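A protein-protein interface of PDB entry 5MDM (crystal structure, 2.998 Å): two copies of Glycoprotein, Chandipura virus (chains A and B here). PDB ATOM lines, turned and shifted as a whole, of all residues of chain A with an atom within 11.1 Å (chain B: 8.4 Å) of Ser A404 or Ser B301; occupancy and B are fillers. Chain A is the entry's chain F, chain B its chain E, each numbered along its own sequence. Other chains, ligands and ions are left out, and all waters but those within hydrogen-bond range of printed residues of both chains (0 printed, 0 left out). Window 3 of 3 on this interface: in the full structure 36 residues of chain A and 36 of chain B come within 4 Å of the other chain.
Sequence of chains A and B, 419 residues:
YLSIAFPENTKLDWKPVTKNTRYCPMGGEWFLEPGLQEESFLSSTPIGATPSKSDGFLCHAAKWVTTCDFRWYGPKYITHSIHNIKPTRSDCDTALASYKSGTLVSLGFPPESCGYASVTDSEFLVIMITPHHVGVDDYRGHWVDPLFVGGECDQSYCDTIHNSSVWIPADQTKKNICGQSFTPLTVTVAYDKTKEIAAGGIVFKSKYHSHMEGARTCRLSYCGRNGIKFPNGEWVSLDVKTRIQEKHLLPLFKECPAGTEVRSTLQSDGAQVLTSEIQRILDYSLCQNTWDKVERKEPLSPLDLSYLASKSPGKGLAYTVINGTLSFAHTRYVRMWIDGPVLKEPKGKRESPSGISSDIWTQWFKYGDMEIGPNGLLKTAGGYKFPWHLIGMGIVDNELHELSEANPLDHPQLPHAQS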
ATOM      1  N   PHE A  31     -10.773 -29.819 -11.963  1.00  0.00           N
ATOM      2  CA  PHE A  31     -11.663 -28.693 -12.197  1.00  0.00           C
ATOM      3  C   PHE A  31     -11.987 -28.510 -13.680  1.00  0.00           C
ATOM      4  O   PHE A  31     -11.146 -28.751 -14.549  1.00  0.00           O
ATOM      5  CB  PHE A  31     -11.036 -27.406 -11.661  1.00  0.00           C
ATOM      6  CG  PHE A  31     -10.668 -27.466 -10.210  1.00  0.00           C
ATOM      7  CD1 PHE A  31      -9.394 -27.837  -9.820  1.00  0.00           C
ATOM      8  CD2 PHE A  31     -11.594 -27.140  -9.234  1.00  0.00           C
ATOM      9  CE1 PHE A  31      -9.053 -27.888  -8.477  1.00  0.00           C
ATOM     10  CE2 PHE A  31     -11.257 -27.189  -7.891  1.00  0.00           C
ATOM     11  CZ  PHE A  31      -9.988 -27.561  -7.512  1.00  0.00           C
ATOM     12  N   LEU A  32     -13.216 -28.090 -13.959  1.00  0.00           N
ATOM     13  CA  LEU A  32     -13.593 -27.651 -15.293  1.00  0.00           C
ATOM     14  C   LEU A  32     -13.846 -26.148 -15.270  1.00  0.00           C
ATOM     15  O   LEU A  32     -14.095 -25.570 -14.212  1.00  0.00           O
ATOM     16  CB  LEU A  32     -14.851 -28.378 -15.767  1.00  0.00           C
ATOM     17  CG  LEU A  32     -14.675 -29.639 -16.613  1.00  0.00           C
ATOM     18  CD1 LEU A  32     -16.035 -30.153 -17.051  1.00  0.00           C
ATOM     19  CD2 LEU A  32     -13.794 -29.359 -17.820  1.00  0.00           C
ATOM     20  N   GLU A  33     -13.779 -25.516 -16.437  1.00  0.00           N
ATOM     21  CA  GLU A  33     -14.083 -24.097 -16.539  1.00  0.00           C
ATOM     22  C   GLU A  33     -15.532 -23.861 -16.132  1.00  0.00           C
ATOM     23  O   GLU A  33     -16.445 -24.480 -16.678  1.00  0.00           O
ATOM     24  CB  GLU A  33     -13.831 -23.589 -17.958  1.00  0.00           C
ATOM     25  CG  GLU A  33     -12.373 -23.635 -18.385  1.00  0.00           C
ATOM     26  CD  GLU A  33     -11.516 -22.616 -17.653  1.00  0.00           C
ATOM     27  OE1 GLU A  33     -12.088 -21.642 -17.110  1.00  0.00           O
ATOM     28  OE2 GLU A  33     -10.274 -22.787 -17.626  1.00  0.00           O
ATOM     29  N   PRO A  34     -15.743 -22.969 -15.155  1.00  0.00           N
ATOM     30  CA  PRO A  34     -17.063 -22.735 -14.556  1.00  0.00           C
ATOM     31  C   PRO A  34     -18.059 -22.021 -15.474  1.00  0.00           C
ATOM     32  O   PRO A  34     -19.263 -22.089 -15.224  1.00  0.00           O
ATOM     33  CB  PRO A  34     -16.741 -21.863 -13.339  1.00  0.00           C
ATOM     34  CG  PRO A  34     -15.474 -21.170 -13.703  1.00  0.00           C
ATOM     35  CD  PRO A  34     -14.694 -22.148 -14.526  1.00  0.00           C
ATOM     36  N   GLY A  35     -17.574 -21.350 -16.514  1.00  0.00           N
ATOM     37  CA  GLY A  35     -18.452 -20.595 -17.393  1.00  0.00           C
ATOM     38  C   GLY A  35     -19.040 -21.414 -18.528  1.00  0.00           C
ATOM     39  O   GLY A  35     -19.557 -20.866 -19.506  1.00  0.00           O
ATOM     40  N   LEU A  36     -18.971 -22.733 -18.391  1.00  0.00           N
ATOM     41  CA  LEU A  36     -19.366 -23.647 -19.456  1.00  0.00           C
ATOM     42  C   LEU A  36     -20.869 -23.881 -19.535  1.00  0.00           C
ATOM     43  O   LEU A  36     -21.531 -24.122 -18.524  1.00  0.00           O
ATOM     44  CB  LEU A  36     -18.647 -24.986 -19.299  1.00  0.00           C
ATOM     45  CG  LEU A  36     -17.398 -25.205 -20.153  1.00  0.00           C
ATOM     46  CD1 LEU A  36     -16.611 -23.911 -20.352  1.00  0.00           C
ATOM     47  CD2 LEU A  36     -16.527 -26.299 -19.543  1.00  0.00           C
ATOM     48  N   GLU A 399     -21.653 -27.986  -6.620  1.00  0.00           N
ATOM     49  CA  GLU A 399     -22.502 -26.819  -6.403  1.00  0.00           C
ATOM     50  C   GLU A 399     -22.178 -25.703  -7.393  1.00  0.00           C
ATOM     51  O   GLU A 399     -21.014 -25.357  -7.590  1.00  0.00           O
ATOM     52  CB  GLU A 399     -22.348 -26.302  -4.973  1.00  0.00           C
ATOM     53  CG  GLU A 399     -23.204 -25.085  -4.655  1.00  0.00           C
ATOM     54  CD  GLU A 399     -24.670 -25.428  -4.484  1.00  0.00           C
ATOM     55  OE1 GLU A 399     -24.973 -26.589  -4.136  1.00  0.00           O
ATOM     56  OE2 GLU A 399     -25.517 -24.536  -4.696  1.00  0.00           O
ATOM     57  N   LEU A 400     -23.214 -25.141  -8.005  1.00  0.00           N
ATOM     58  CA  LEU A 400     -23.038 -24.083  -8.998  1.00  0.00           C
ATOM     59  C   LEU A 400     -23.084 -22.687  -8.372  1.00  0.00           C
ATOM     60  O   LEU A 400     -22.627 -21.714  -8.975  1.00  0.00           O
ATOM     61  CB  LEU A 400     -24.085 -24.195 -10.115  1.00  0.00           C
ATOM     62  CG  LEU A 400     -23.883 -25.253 -11.205  1.00  0.00           C
ATOM     63  CD1 LEU A 400     -24.056 -26.674 -10.669  1.00  0.00           C
ATOM     64  CD2 LEU A 400     -24.830 -24.996 -12.371  1.00  0.00           C
ATOM     65  N   HIS A 401     -23.639 -22.595  -7.166  1.00  0.00           N
ATOM     66  CA  HIS A 401     -23.702 -21.330  -6.439  1.00  0.00           C
ATOM     67  C   HIS A 401     -22.301 -20.829  -6.105  1.00  0.00           C
ATOM     68  O   HIS A 401     -22.042 -19.624  -6.101  1.00  0.00           O
ATOM     69  CB  HIS A 401     -24.512 -21.487  -5.148  1.00  0.00           C
ATOM     70  CG  HIS A 401     -25.997 -21.485  -5.354  1.00  0.00           C
ATOM     71  ND1 HIS A 401     -26.606 -22.139  -6.404  1.00  0.00           N
ATOM     72  CD2 HIS A 401     -26.994 -20.915  -4.636  1.00  0.00           C
ATOM     73  CE1 HIS A 401     -27.914 -21.967  -6.327  1.00  0.00           C
ATOM     74  NE2 HIS A 401     -28.175 -21.227  -5.264  1.00  0.00           N
ATOM     75  N   GLU A 402     -21.401 -21.771  -5.831  1.00  0.00           N
ATOM     76  CA  GLU A 402     -20.034 -21.462  -5.428  1.00  0.00           C
ATOM     77  C   GLU A 402     -19.206 -20.886  -6.569  1.00  0.00           C
ATOM     78  O   GLU A 402     -18.191 -20.230  -6.336  1.00  0.00           O
ATOM     79  CB  GLU A 402     -19.347 -22.723  -4.901  1.00  0.00           C
ATOM     80  CG  GLU A 402     -20.142 -23.487  -3.859  1.00  0.00           C
ATOM     81  CD  GLU A 402     -20.105 -22.842  -2.487  1.00  0.00           C
ATOM     82  OE1 GLU A 402     -19.641 -21.689  -2.368  1.00  0.00           O
ATOM     83  OE2 GLU A 402     -20.539 -23.498  -1.519  1.00  0.00           O
ATOM     84  N   LEU A 403     -19.642 -21.144  -7.798  1.00  0.00           N
ATOM     85  CA  LEU A 403     -18.915 -20.721  -8.989  1.00  0.00           C
ATOM     86  C   LEU A 403     -19.745 -19.747  -9.815  1.00  0.00           C
ATOM     87  O   LEU A 403     -20.391 -20.144 -10.783  1.00  0.00           O
ATOM     88  CB  LEU A 403     -18.555 -21.943  -9.839  1.00  0.00           C
ATOM     89  CG  LEU A 403     -17.686 -23.002  -9.160  1.00  0.00           C
ATOM     90  CD1 LEU A 403     -18.075 -24.396  -9.612  1.00  0.00           C
ATOM     91  CD2 LEU A 403     -16.213 -22.735  -9.447  1.00  0.00           C
ATOM     92  N   SER A 404     -19.727 -18.471  -9.436  1.00  0.00           N
ATOM     93  CA  SER A 404     -20.522 -17.467 -10.137  1.00  0.00           C
ATOM     94  C   SER A 404     -20.018 -16.043  -9.920  1.00  0.00           C
ATOM     95  O   SER A 404     -19.534 -15.707  -8.837  1.00  0.00           O
ATOM     96  CB  SER A 404     -21.987 -17.557  -9.708  1.00  0.00           C
ATOM     97  OG  SER A 404     -22.122 -17.291  -8.322  1.00  0.00           O
ATOM     98  N   GLU A 405     -20.145 -15.220 -10.960  1.00  0.00           N
ATOM     99  CA  GLU A 405     -19.848 -13.790 -10.892  1.00  0.00           C
ATOM    100  C   GLU A 405     -18.409 -13.515 -10.458  1.00  0.00           C
ATOM    101  O   GLU A 405     -18.124 -12.497  -9.826  1.00  0.00           O
ATOM    102  CB  GLU A 405     -20.834 -13.084  -9.956  1.00  0.00           C
ATOM    103  CG  GLU A 405     -21.057 -11.612 -10.263  1.00  0.00           C
ATOM    104  CD  GLU A 405     -22.065 -10.974  -9.328  1.00  0.00           C
ATOM    105  OE1 GLU A 405     -22.299 -11.529  -8.234  1.00  0.00           O
ATOM    106  OE2 GLU A 405     -22.631  -9.919  -9.688  1.00  0.00           O
ATOM    107  N   THR B 290      -6.382 -17.473  -7.340  1.00  0.00           N
ATOM    108  CA  THR B 290      -7.409 -16.493  -7.016  1.00  0.00           C
ATOM    109  C   THR B 290      -6.856 -15.067  -7.090  1.00  0.00           C
ATOM    110  O   THR B 290      -7.473 -14.181  -7.689  1.00  0.00           O
ATOM    111  CB  THR B 290      -8.019 -16.746  -5.623  1.00  0.00           C
ATOM    112  OG1 THR B 290      -8.863 -17.898  -5.687  1.00  0.00           O
ATOM    113  CG2 THR B 290      -8.847 -15.542  -5.155  1.00  0.00           C
ATOM    114  N   LYS B 293      -6.610 -14.001 -10.484  1.00  0.00           N
ATOM    115  CA  LYS B 293      -7.901 -13.559 -11.001  1.00  0.00           C
ATOM    116  C   LYS B 293      -8.144 -12.117 -10.588  1.00  0.00           C
ATOM    117  O   LYS B 293      -8.607 -11.305 -11.391  1.00  0.00           O
ATOM    118  CB  LYS B 293      -9.046 -14.457 -10.524  1.00  0.00           C
ATOM    119  CG  LYS B 293      -9.060 -15.834 -11.170  1.00  0.00           C
ATOM    120  CD  LYS B 293     -10.283 -16.640 -10.769  1.00  0.00           C
ATOM    121  CE  LYS B 293     -10.185 -18.074 -11.281  1.00  0.00           C
ATOM    122  NZ  LYS B 293     -11.316 -18.928 -10.810  1.00  0.00           N
ATOM    123  N   GLU B 298     -10.517 -10.013 -13.077  1.00  0.00           N
ATOM    124  CA  GLU B 298     -11.599 -10.957 -13.317  1.00  0.00           C
ATOM    125  C   GLU B 298     -12.515 -10.978 -12.098  1.00  0.00           C
ATOM    126  O   GLU B 298     -12.082 -10.683 -10.984  1.00  0.00           O
ATOM    127  CB  GLU B 298     -11.038 -12.354 -13.602  1.00  0.00           C
ATOM    128  CG  GLU B 298     -10.154 -12.428 -14.843  1.00  0.00           C
ATOM    129  CD  GLU B 298      -9.542 -13.806 -15.062  1.00  0.00           C
ATOM    130  OE1 GLU B 298      -9.903 -14.749 -14.325  1.00  0.00           O
ATOM    131  OE2 GLU B 298      -8.696 -13.944 -15.972  1.00  0.00           O
ATOM    132  N   PRO B 299     -13.796 -11.311 -12.306  1.00  0.00           N
ATOM    133  CA  PRO B 299     -14.725 -11.381 -11.177  1.00  0.00           C
ATOM    134  C   PRO B 299     -14.420 -12.594 -10.303  1.00  0.00           C
ATOM    135  O   PRO B 299     -13.821 -13.556 -10.785  1.00  0.00           O
ATOM    136  CB  PRO B 299     -16.078 -11.539 -11.865  1.00  0.00           C
ATOM    137  CG  PRO B 299     -15.760 -12.224 -13.143  1.00  0.00           C
ATOM    138  CD  PRO B 299     -14.451 -11.645 -13.582  1.00  0.00           C
ATOM    139  N   LEU B 300     -14.821 -12.546  -9.035  1.00  0.00           N
ATOM    140  CA  LEU B 300     -14.536 -13.638  -8.112  1.00  0.00           C
ATOM    141  C   LEU B 300     -15.784 -14.399  -7.691  1.00  0.00           C
ATOM    142  O   LEU B 300     -16.818 -13.802  -7.383  1.00  0.00           O
ATOM    143  CB  LEU B 300     -13.826 -13.116  -6.865  1.00  0.00           C
ATOM    144  CG  LEU B 300     -12.398 -12.609  -7.026  1.00  0.00           C
ATOM    145  CD1 LEU B 300     -11.839 -12.255  -5.658  1.00  0.00           C
ATOM    146  CD2 LEU B 300     -11.536 -13.651  -7.721  1.00  0.00           C
ATOM    147  N   SER B 301     -15.674 -15.723  -7.671  1.00  0.00           N
ATOM    148  CA  SER B 301     -16.739 -16.575  -7.165  1.00  0.00           C
ATOM    149  C   SER B 301     -16.504 -16.817  -5.675  1.00  0.00           C
ATOM    150  O   SER B 301     -15.393 -16.615  -5.189  1.00  0.00           O
ATOM    151  CB  SER B 301     -16.753 -17.900  -7.926  1.00  0.00           C
ATOM    152  OG  SER B 301     -15.700 -18.742  -7.499  1.00  0.00           O
ATOM    153  N   PRO B 302     -17.553 -17.229  -4.939  1.00  0.00           N
ATOM    154  CA  PRO B 302     -17.385 -17.573  -3.524  1.00  0.00           C
ATOM    155  C   PRO B 302     -16.250 -18.570  -3.297  1.00  0.00           C
ATOM    156  O   PRO B 302     -15.522 -18.454  -2.310  1.00  0.00           O
ATOM    157  CB  PRO B 302     -18.728 -18.213  -3.169  1.00  0.00           C
ATOM    158  CG  PRO B 302     -19.699 -17.520  -4.052  1.00  0.00           C
ATOM    159  CD  PRO B 302     -18.971 -17.254  -5.344  1.00  0.00           C
ATOM    160  N   LEU B 303     -16.097 -19.523  -4.212  1.00  0.00           N
ATOM    161  CA  LEU B 303     -15.061 -20.544  -4.099  1.00  0.00           C
ATOM    162  C   LEU B 303     -13.663 -19.921  -4.188  1.00  0.00           C
ATOM    163  O   LEU B 303     -12.754 -20.243  -3.394  1.00  0.00           O
ATOM    164  CB  LEU B 303     -15.255 -21.601  -5.187  1.00  0.00           C
ATOM    165  CG  LEU B 303     -14.388 -22.858  -5.100  1.00  0.00           C
ATOM    166  CD1 LEU B 303     -14.422 -23.445  -3.696  1.00  0.00           C
ATOM    167  CD2 LEU B 303     -14.857 -23.885  -6.115  1.00  0.00           C
ATOM    168  N   ASP B 304     -13.506 -19.020  -5.156  1.00  0.00           N
ATOM    169  CA  ASP B 304     -12.276 -18.253  -5.313  1.00  0.00           C
ATOM    170  C   ASP B 304     -11.947 -17.528  -4.015  1.00  0.00           C
ATOM    171  O   ASP B 304     -10.795 -17.482  -3.596  1.00  0.00           O
ATOM    172  CB  ASP B 304     -12.409 -17.232  -6.447  1.00  0.00           C
ATOM    173  CG  ASP B 304     -12.672 -17.874  -7.797  1.00  0.00           C
ATOM    174  OD1 ASP B 304     -12.210 -19.017  -8.028  1.00  0.00           O
ATOM    175  OD2 ASP B 304     -13.339 -17.222  -8.634  1.00  0.00           O
ATOM    176  N   LEU B 305     -12.970 -16.962  -3.382  1.00  0.00           N
ATOM    177  CA  LEU B 305     -12.798 -16.301  -2.098  1.00  0.00           C
ATOM    178  C   LEU B 305     -12.340 -17.281  -1.018  1.00  0.00           C
ATOM    179  O   LEU B 305     -11.494 -16.955  -0.183  1.00  0.00           O
ATOM    180  CB  LEU B 305     -14.098 -15.633  -1.677  1.00  0.00           C
ATOM    181  CG  LEU B 305     -14.385 -14.335  -2.412  1.00  0.00           C
ATOM    182  CD1 LEU B 305     -15.742 -13.806  -1.989  1.00  0.00           C
ATOM    183  CD2 LEU B 305     -13.279 -13.330  -2.124  1.00  0.00           C
ATOM    184  N   SER B 306     -12.901 -18.482  -1.042  1.00  0.00           N
ATOM    185  CA  SER B 306     -12.584 -19.482  -0.038  1.00  0.00           C
ATOM    186  C   SER B 306     -11.148 -19.958  -0.162  1.00  0.00           C
ATOM    187  O   SER B 306     -10.561 -20.425   0.811  1.00  0.00           O
ATOM    188  CB  SER B 306     -13.521 -20.669  -0.167  1.00  0.00           C
ATOM    189  OG  SER B 306     -13.285 -21.361  -1.379  1.00  0.00           O
ATOM    190  N   TYR B 307     -10.579 -19.847  -1.357  1.00  0.00           N
ATOM    191  CA  TYR B 307      -9.163 -20.189  -1.520  1.00  0.00           C
ATOM    192  C   TYR B 307      -8.230 -19.231  -0.768  1.00  0.00           C
ATOM    193  O   TYR B 307      -7.031 -19.480  -0.662  1.00  0.00           O
ATOM    194  CB  TYR B 307      -8.778 -20.284  -3.001  1.00  0.00           C
ATOM    195  CG  TYR B 307      -9.432 -21.450  -3.708  1.00  0.00           C
ATOM    196  CD1 TYR B 307      -9.681 -22.636  -3.032  1.00  0.00           C
ATOM    197  CD2 TYR B 307      -9.820 -21.359  -5.038  1.00  0.00           C
ATOM    198  CE1 TYR B 307     -10.286 -23.704  -3.664  1.00  0.00           C
ATOM    199  CE2 TYR B 307     -10.428 -22.424  -5.678  1.00  0.00           C
ATOM    200  CZ  TYR B 307     -10.658 -23.594  -4.985  1.00  0.00           C
ATOM    201  OH  TYR B 307     -11.261 -24.660  -5.607  1.00  0.00           O
ATOM    202  N   LEU B 308      -8.787 -18.149  -0.234  1.00  0.00           N
ATOM    203  CA  LEU B 308      -8.008 -17.147   0.485  1.00  0.00           C
ATOM    204  C   LEU B 308      -8.134 -17.348   1.985  1.00  0.00           C
ATOM    205  O   LEU B 308      -7.391 -16.756   2.766  1.00  0.00           O
ATOM    206  CB  LEU B 308      -8.489 -15.737   0.133  1.00  0.00           C
ATOM    207  CG  LEU B 308      -8.471 -15.305  -1.332  1.00  0.00           C
ATOM    208  CD1 LEU B 308      -8.967 -13.886  -1.458  1.00  0.00           C
ATOM    209  CD2 LEU B 308      -7.075 -15.432  -1.898  1.00  0.00           C
ATOM    210  N   THR B 320     -14.087 -10.836   1.410  1.00  0.00           N
ATOM    211  CA  THR B 320     -15.452 -10.930   0.905  1.00  0.00           C
ATOM    212  C   THR B 320     -15.667  -9.934  -0.226  1.00  0.00           C
ATOM    213  O   THR B 320     -14.761  -9.178  -0.575  1.00  0.00           O
ATOM    214  CB  THR B 320     -16.498 -10.700   2.020  1.00  0.00           C
ATOM    215  OG1 THR B 320     -17.796 -11.072   1.543  1.00  0.00           O
ATOM    216  CG2 THR B 320     -16.518  -9.242   2.460  1.00  0.00           C
ATOM    217  N   VAL B 321     -16.862  -9.943  -0.807  1.00  0.00           N
ATOM    218  CA  VAL B 321     -17.188  -9.013  -1.883  1.00  0.00           C
ATOM    219  C   VAL B 321     -18.374  -8.126  -1.508  1.00  0.00           C
ATOM    220  O   VAL B 321     -19.532  -8.534  -1.613  1.00  0.00           O
ATOM    221  CB  VAL B 321     -17.476  -9.747  -3.212  1.00  0.00           C
ATOM    222  CG1 VAL B 321     -17.719  -8.748  -4.322  1.00  0.00           C
ATOM    223  CG2 VAL B 321     -16.314 -10.647  -3.578  1.00  0.00           C
ATOM    224  N   LEU B 326     -13.771  -6.091  -3.678  1.00  0.00           N
ATOM    225  CA  LEU B 326     -12.985  -6.985  -2.837  1.00  0.00           C
ATOM    226  C   LEU B 326     -12.598  -6.290  -1.541  1.00  0.00           C
ATOM    227  O   LEU B 326     -11.911  -5.266  -1.550  1.00  0.00           O
ATOM    228  CB  LEU B 326     -11.724  -7.452  -3.562  1.00  0.00           C
ATOM    229  CG  LEU B 326     -10.887  -8.503  -2.826  1.00  0.00           C
ATOM    230  CD1 LEU B 326     -11.574  -9.864  -2.853  1.00  0.00           C
ATOM    231  CD2 LEU B 326      -9.483  -8.593  -3.407  1.00  0.00           C
ATOM    232  N   TYR B 367     -24.840  -9.941  -2.251  1.00  0.00           N
ATOM    233  CA  TYR B 367     -24.013 -10.545  -3.292  1.00  0.00           C
ATOM    234  C   TYR B 367     -24.893 -11.123  -4.393  1.00  0.00           C
ATOM    235  O   TYR B 367     -25.143 -12.330  -4.439  1.00  0.00           O
ATOM    236  CB  TYR B 367     -23.116 -11.630  -2.693  1.00  0.00           C
ATOM    237  CG  TYR B 367     -22.218 -12.332  -3.690  1.00  0.00           C
ATOM    238  CD1 TYR B 367     -21.092 -11.701  -4.206  1.00  0.00           C
ATOM    239  CD2 TYR B 367     -22.485 -13.633  -4.098  1.00  0.00           C
ATOM    240  CE1 TYR B 367     -20.271 -12.342  -5.113  1.00  0.00           C
ATOM    241  CE2 TYR B 367     -21.671 -14.280  -5.003  1.00  0.00           C
ATOM    242  CZ  TYR B 367     -20.567 -13.632  -5.508  1.00  0.00           C
ATOM    243  OH  TYR B 367     -19.757 -14.281  -6.411  1.00  0.00           O
ATOM    244  N   GLY B 368     -25.368 -10.250  -5.275  1.00  0.00           N
ATOM    245  CA  GLY B 368     -26.304 -10.645  -6.311  1.00  0.00           C
ATOM    246  C   GLY B 368     -27.678 -10.923  -5.731  1.00  0.00           C
ATOM    247  O   GLY B 368     -28.256 -10.076  -5.048  1.00  0.00           O
ATOM    248  N   ASP B 369     -28.195 -12.118  -5.997  1.00  0.00           N
ATOM    249  CA  ASP B 369     -29.503 -12.526  -5.496  1.00  0.00           C
ATOM    250  C   ASP B 369     -29.433 -12.995  -4.042  1.00  0.00           C
ATOM    251  O   ASP B 369     -30.443 -13.015  -3.335  1.00  0.00           O
ATOM    252  CB  ASP B 369     -30.076 -13.641  -6.375  1.00  0.00           C
ATOM    253  CG  ASP B 369     -29.113 -14.805  -6.543  1.00  0.00           C
ATOM    254  OD1 ASP B 369     -27.902 -14.557  -6.726  1.00  0.00           O
ATOM    255  OD2 ASP B 369     -29.566 -15.968  -6.488  1.00  0.00           O
ATOM    256  N   MET B 370     -28.234 -13.369  -3.604  1.00  0.00           N
ATOM    257  CA  MET B 370     -28.038 -13.947  -2.278  1.00  0.00           C
ATOM    258  C   MET B 370     -27.065 -13.135  -1.429  1.00  0.00           C
ATOM    259  O   MET B 370     -26.429 -12.201  -1.915  1.00  0.00           O
ATOM    260  CB  MET B 370     -27.542 -15.388  -2.406  1.00  0.00           C
ATOM    261  CG  MET B 370     -26.379 -15.548  -3.365  1.00  0.00           C
ATOM    262  SD  MET B 370     -26.138 -17.260  -3.867  1.00  0.00           S
ATOM    263  CE  MET B 370     -27.728 -17.603  -4.617  1.00  0.00           C
ATOM    264  N   ILE B 372     -23.607 -12.946   1.000  1.00  0.00           N
ATOM    265  CA  ILE B 372     -22.312 -13.596   1.143  1.00  0.00           C
ATOM    266  C   ILE B 372     -21.601 -13.103   2.399  1.00  0.00           C
ATOM    267  O   ILE B 372     -21.834 -11.981   2.866  1.00  0.00           O
ATOM    268  CB  ILE B 372     -21.417 -13.363  -0.098  1.00  0.00           C
ATOM    269  CG1 ILE B 372     -20.433 -14.514  -0.286  1.00  0.00           C
ATOM    270  CG2 ILE B 372     -20.689 -12.027  -0.010  1.00  0.00           C
ATOM    271  CD1 ILE B 372     -19.557 -14.358  -1.506  1.00  0.00           C
ATOM    272  N   ASN B 375     -14.879 -15.163   3.227  1.00  0.00           N
ATOM    273  CA  ASN B 375     -14.279 -16.264   2.483  1.00  0.00           C
ATOM    274  C   ASN B 375     -15.284 -17.108   1.708  1.00  0.00           C
ATOM    275  O   ASN B 375     -15.194 -18.341   1.695  1.00  0.00           O
ATOM    276  CB  ASN B 375     -13.473 -17.157   3.422  1.00  0.00           C
ATOM    277  CG  ASN B 375     -12.567 -16.366   4.341  1.00  0.00           C
ATOM    278  OD1 ASN B 375     -12.072 -15.297   3.978  1.00  0.00           O
ATOM    279  ND2 ASN B 375     -12.347 -16.887   5.544  1.00  0.00           N
ATOM    280  N   GLY B 376     -16.245 -16.440   1.075  1.00  0.00           N
ATOM    281  CA  GLY B 376     -17.215 -17.108   0.226  1.00  0.00           C
ATOM    282  C   GLY B 376     -18.227 -17.964   0.966  1.00  0.00           C
ATOM    283  O   GLY B 376     -18.681 -18.990   0.458  1.00  0.00           O
ATOM    284  N   LEU B 377     -18.577 -17.551   2.178  1.00  0.00           N
ATOM    285  CA  LEU B 377     -19.644 -18.212   2.910  1.00  0.00           C
ATOM    286  C   LEU B 377     -20.956 -17.773   2.286  1.00  0.00           C
ATOM    287  O   LEU B 377     -21.228 -16.575   2.192  1.00  0.00           O
ATOM    288  CB  LEU B 377     -19.599 -17.828   4.387  1.00  0.00           C
ATOM    289  CG  LEU B 377     -20.701 -18.409   5.276  1.00  0.00           C
ATOM    290  CD1 LEU B 377     -20.831 -19.907   5.062  1.00  0.00           C
ATOM    291  CD2 LEU B 377     -20.419 -18.098   6.735  1.00  0.00           C
ATOM    292  N   LEU B 378     -21.768 -18.729   1.844  1.00  0.00           N
ATOM    293  CA  LEU B 378     -23.003 -18.362   1.155  1.00  0.00           C
ATOM    294  C   LEU B 378     -24.265 -18.447   2.008  1.00  0.00           C
ATOM    295  O   LEU B 378     -24.486 -19.427   2.714  1.00  0.00           O
ATOM    296  CB  LEU B 378     -23.178 -19.170  -0.132  1.00  0.00           C
ATOM    297  CG  LEU B 378     -22.542 -18.530  -1.366  1.00  0.00           C
ATOM    298  CD1 LEU B 378     -22.887 -19.319  -2.614  1.00  0.00           C
ATOM    299  CD2 LEU B 378     -22.977 -17.074  -1.507  1.00  0.00           C
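OH of Tyr B367 sits at hydrogen-bond distance from O of Leu B300, 3.1 Å away. OG of Ser B301 lies close to N of Leu B303 (3.4 Å). The backbone NH of Ser B301 sits at hydrogen-bond distance from the side-chain carboxylate of Asp B304 (2.9 Å). The side-chain hydroxyl of Ser A404 sits at hydrogen-bond distance from the backbone carbonyl oxygen of His A401, at 3.2 Å. The side-chain carboxylate of Glu A399 is in hydrogen-bond range of a ring nitrogen (ND1) of His A401, at 3.1 Å.
No position is printed for both chains.
Printed residues of chain B that touch a printed residue of chain A: Pro B299, Leu B300, Ser B301, Pro B302, Leu B303, Tyr B307, Tyr B367, Met B370 and Leu B378. Hydrophobic or aromatic side chains of chain A that line the printed part of chain B: Phe A31, His A401 and Leu A403. Along chain A the printed residues that touch a printed residue of chain B span positions 31 to 405. Among the printed residues, no Asp or Glu carboxylate lies within 4 Å of a Lys or Arg side-chain nitrogen of the other chain.
Phe A31 touches Tyr B307 (CE2 to OH, 3.4 Å). His A401 touches Pro B302. His A401 touches Met B370 (CD2 to CE, 3.4 Å). O of His A401 touches CD1 of Leu B378 (3.6 Å). Ser B301 touches Leu A403. Leu B303 touches Leu A403. O of Ser A404 touches O of Leu B300 (3.6 Å). O of Ser A404 touches CA of Ser B301 (3.4 Å). Ser A404 touches Pro B302 (O to CD, 3.9 Å). Tyr B367 touches Glu A405.
Of chain B, only Leu B300, Ser B301, Pro B302 and Tyr B367 come within 4 Å of Ser A404. Of chain A, only Glu A402 (3.1 Å), Leu A403 (3.7 Å) and Ser A404 (3.4 Å) come within 4 Å of Ser B301. No residue of chain A comes within 4 Å of Asp B304. No residue of chain A comes within 4 Å of Leu B305. Gly B376 touches none of the printed residues of chain A. Printed residues of chain B within 4 Å of Glu A402: Ser B301 (3.1 Å), Pro B302 (3.2 Å) and Leu B303 (3.1 Å). Printed residues of chain B within 4 Å of His A401: Pro B302 (3.8 Å), Met B370 (3.4 Å) and Leu B378 (3.6 Å). Of the printed residues of chain A, Met B370 touches His A401 (3.4 Å). Of the printed residues of chain A, Leu B378 touches His A401. Of the printed residues of chain B, Leu A403 touches Ser B301 and Leu B303. The nearest residue of chain A that does not touch Ser B301 is Glu A405 (4.5 Å). The nearest printed residue of chain A that does not touch Tyr B367 is His A401 (5.5 Å).
The backbone NH (N) of Leu B303 is in hydrogen-bond range of the backbone carbonyl oxygen (O) of Glu A402, 3.1 Å away. The side-chain hydroxyl of Tyr B367 is in hydrogen-bond range of the backbone carbonyl oxygen of Ser A404 (2.8 Å). The backbone carbonyl oxygen of Glu A402 lies close to the backbone nitrogen of Pro B302 (3.4 Å). The backbone NH (N) of Leu B300 is in hydrogen-bond range of the backbone carbonyl oxygen (O) of Glu A405 (3.4 Å). The side-chain hydroxyl (OG) of Ser B301 lies within hydrogen-bond range of the backbone carbonyl oxygen (O) of Glu A402 (3.1 Å).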
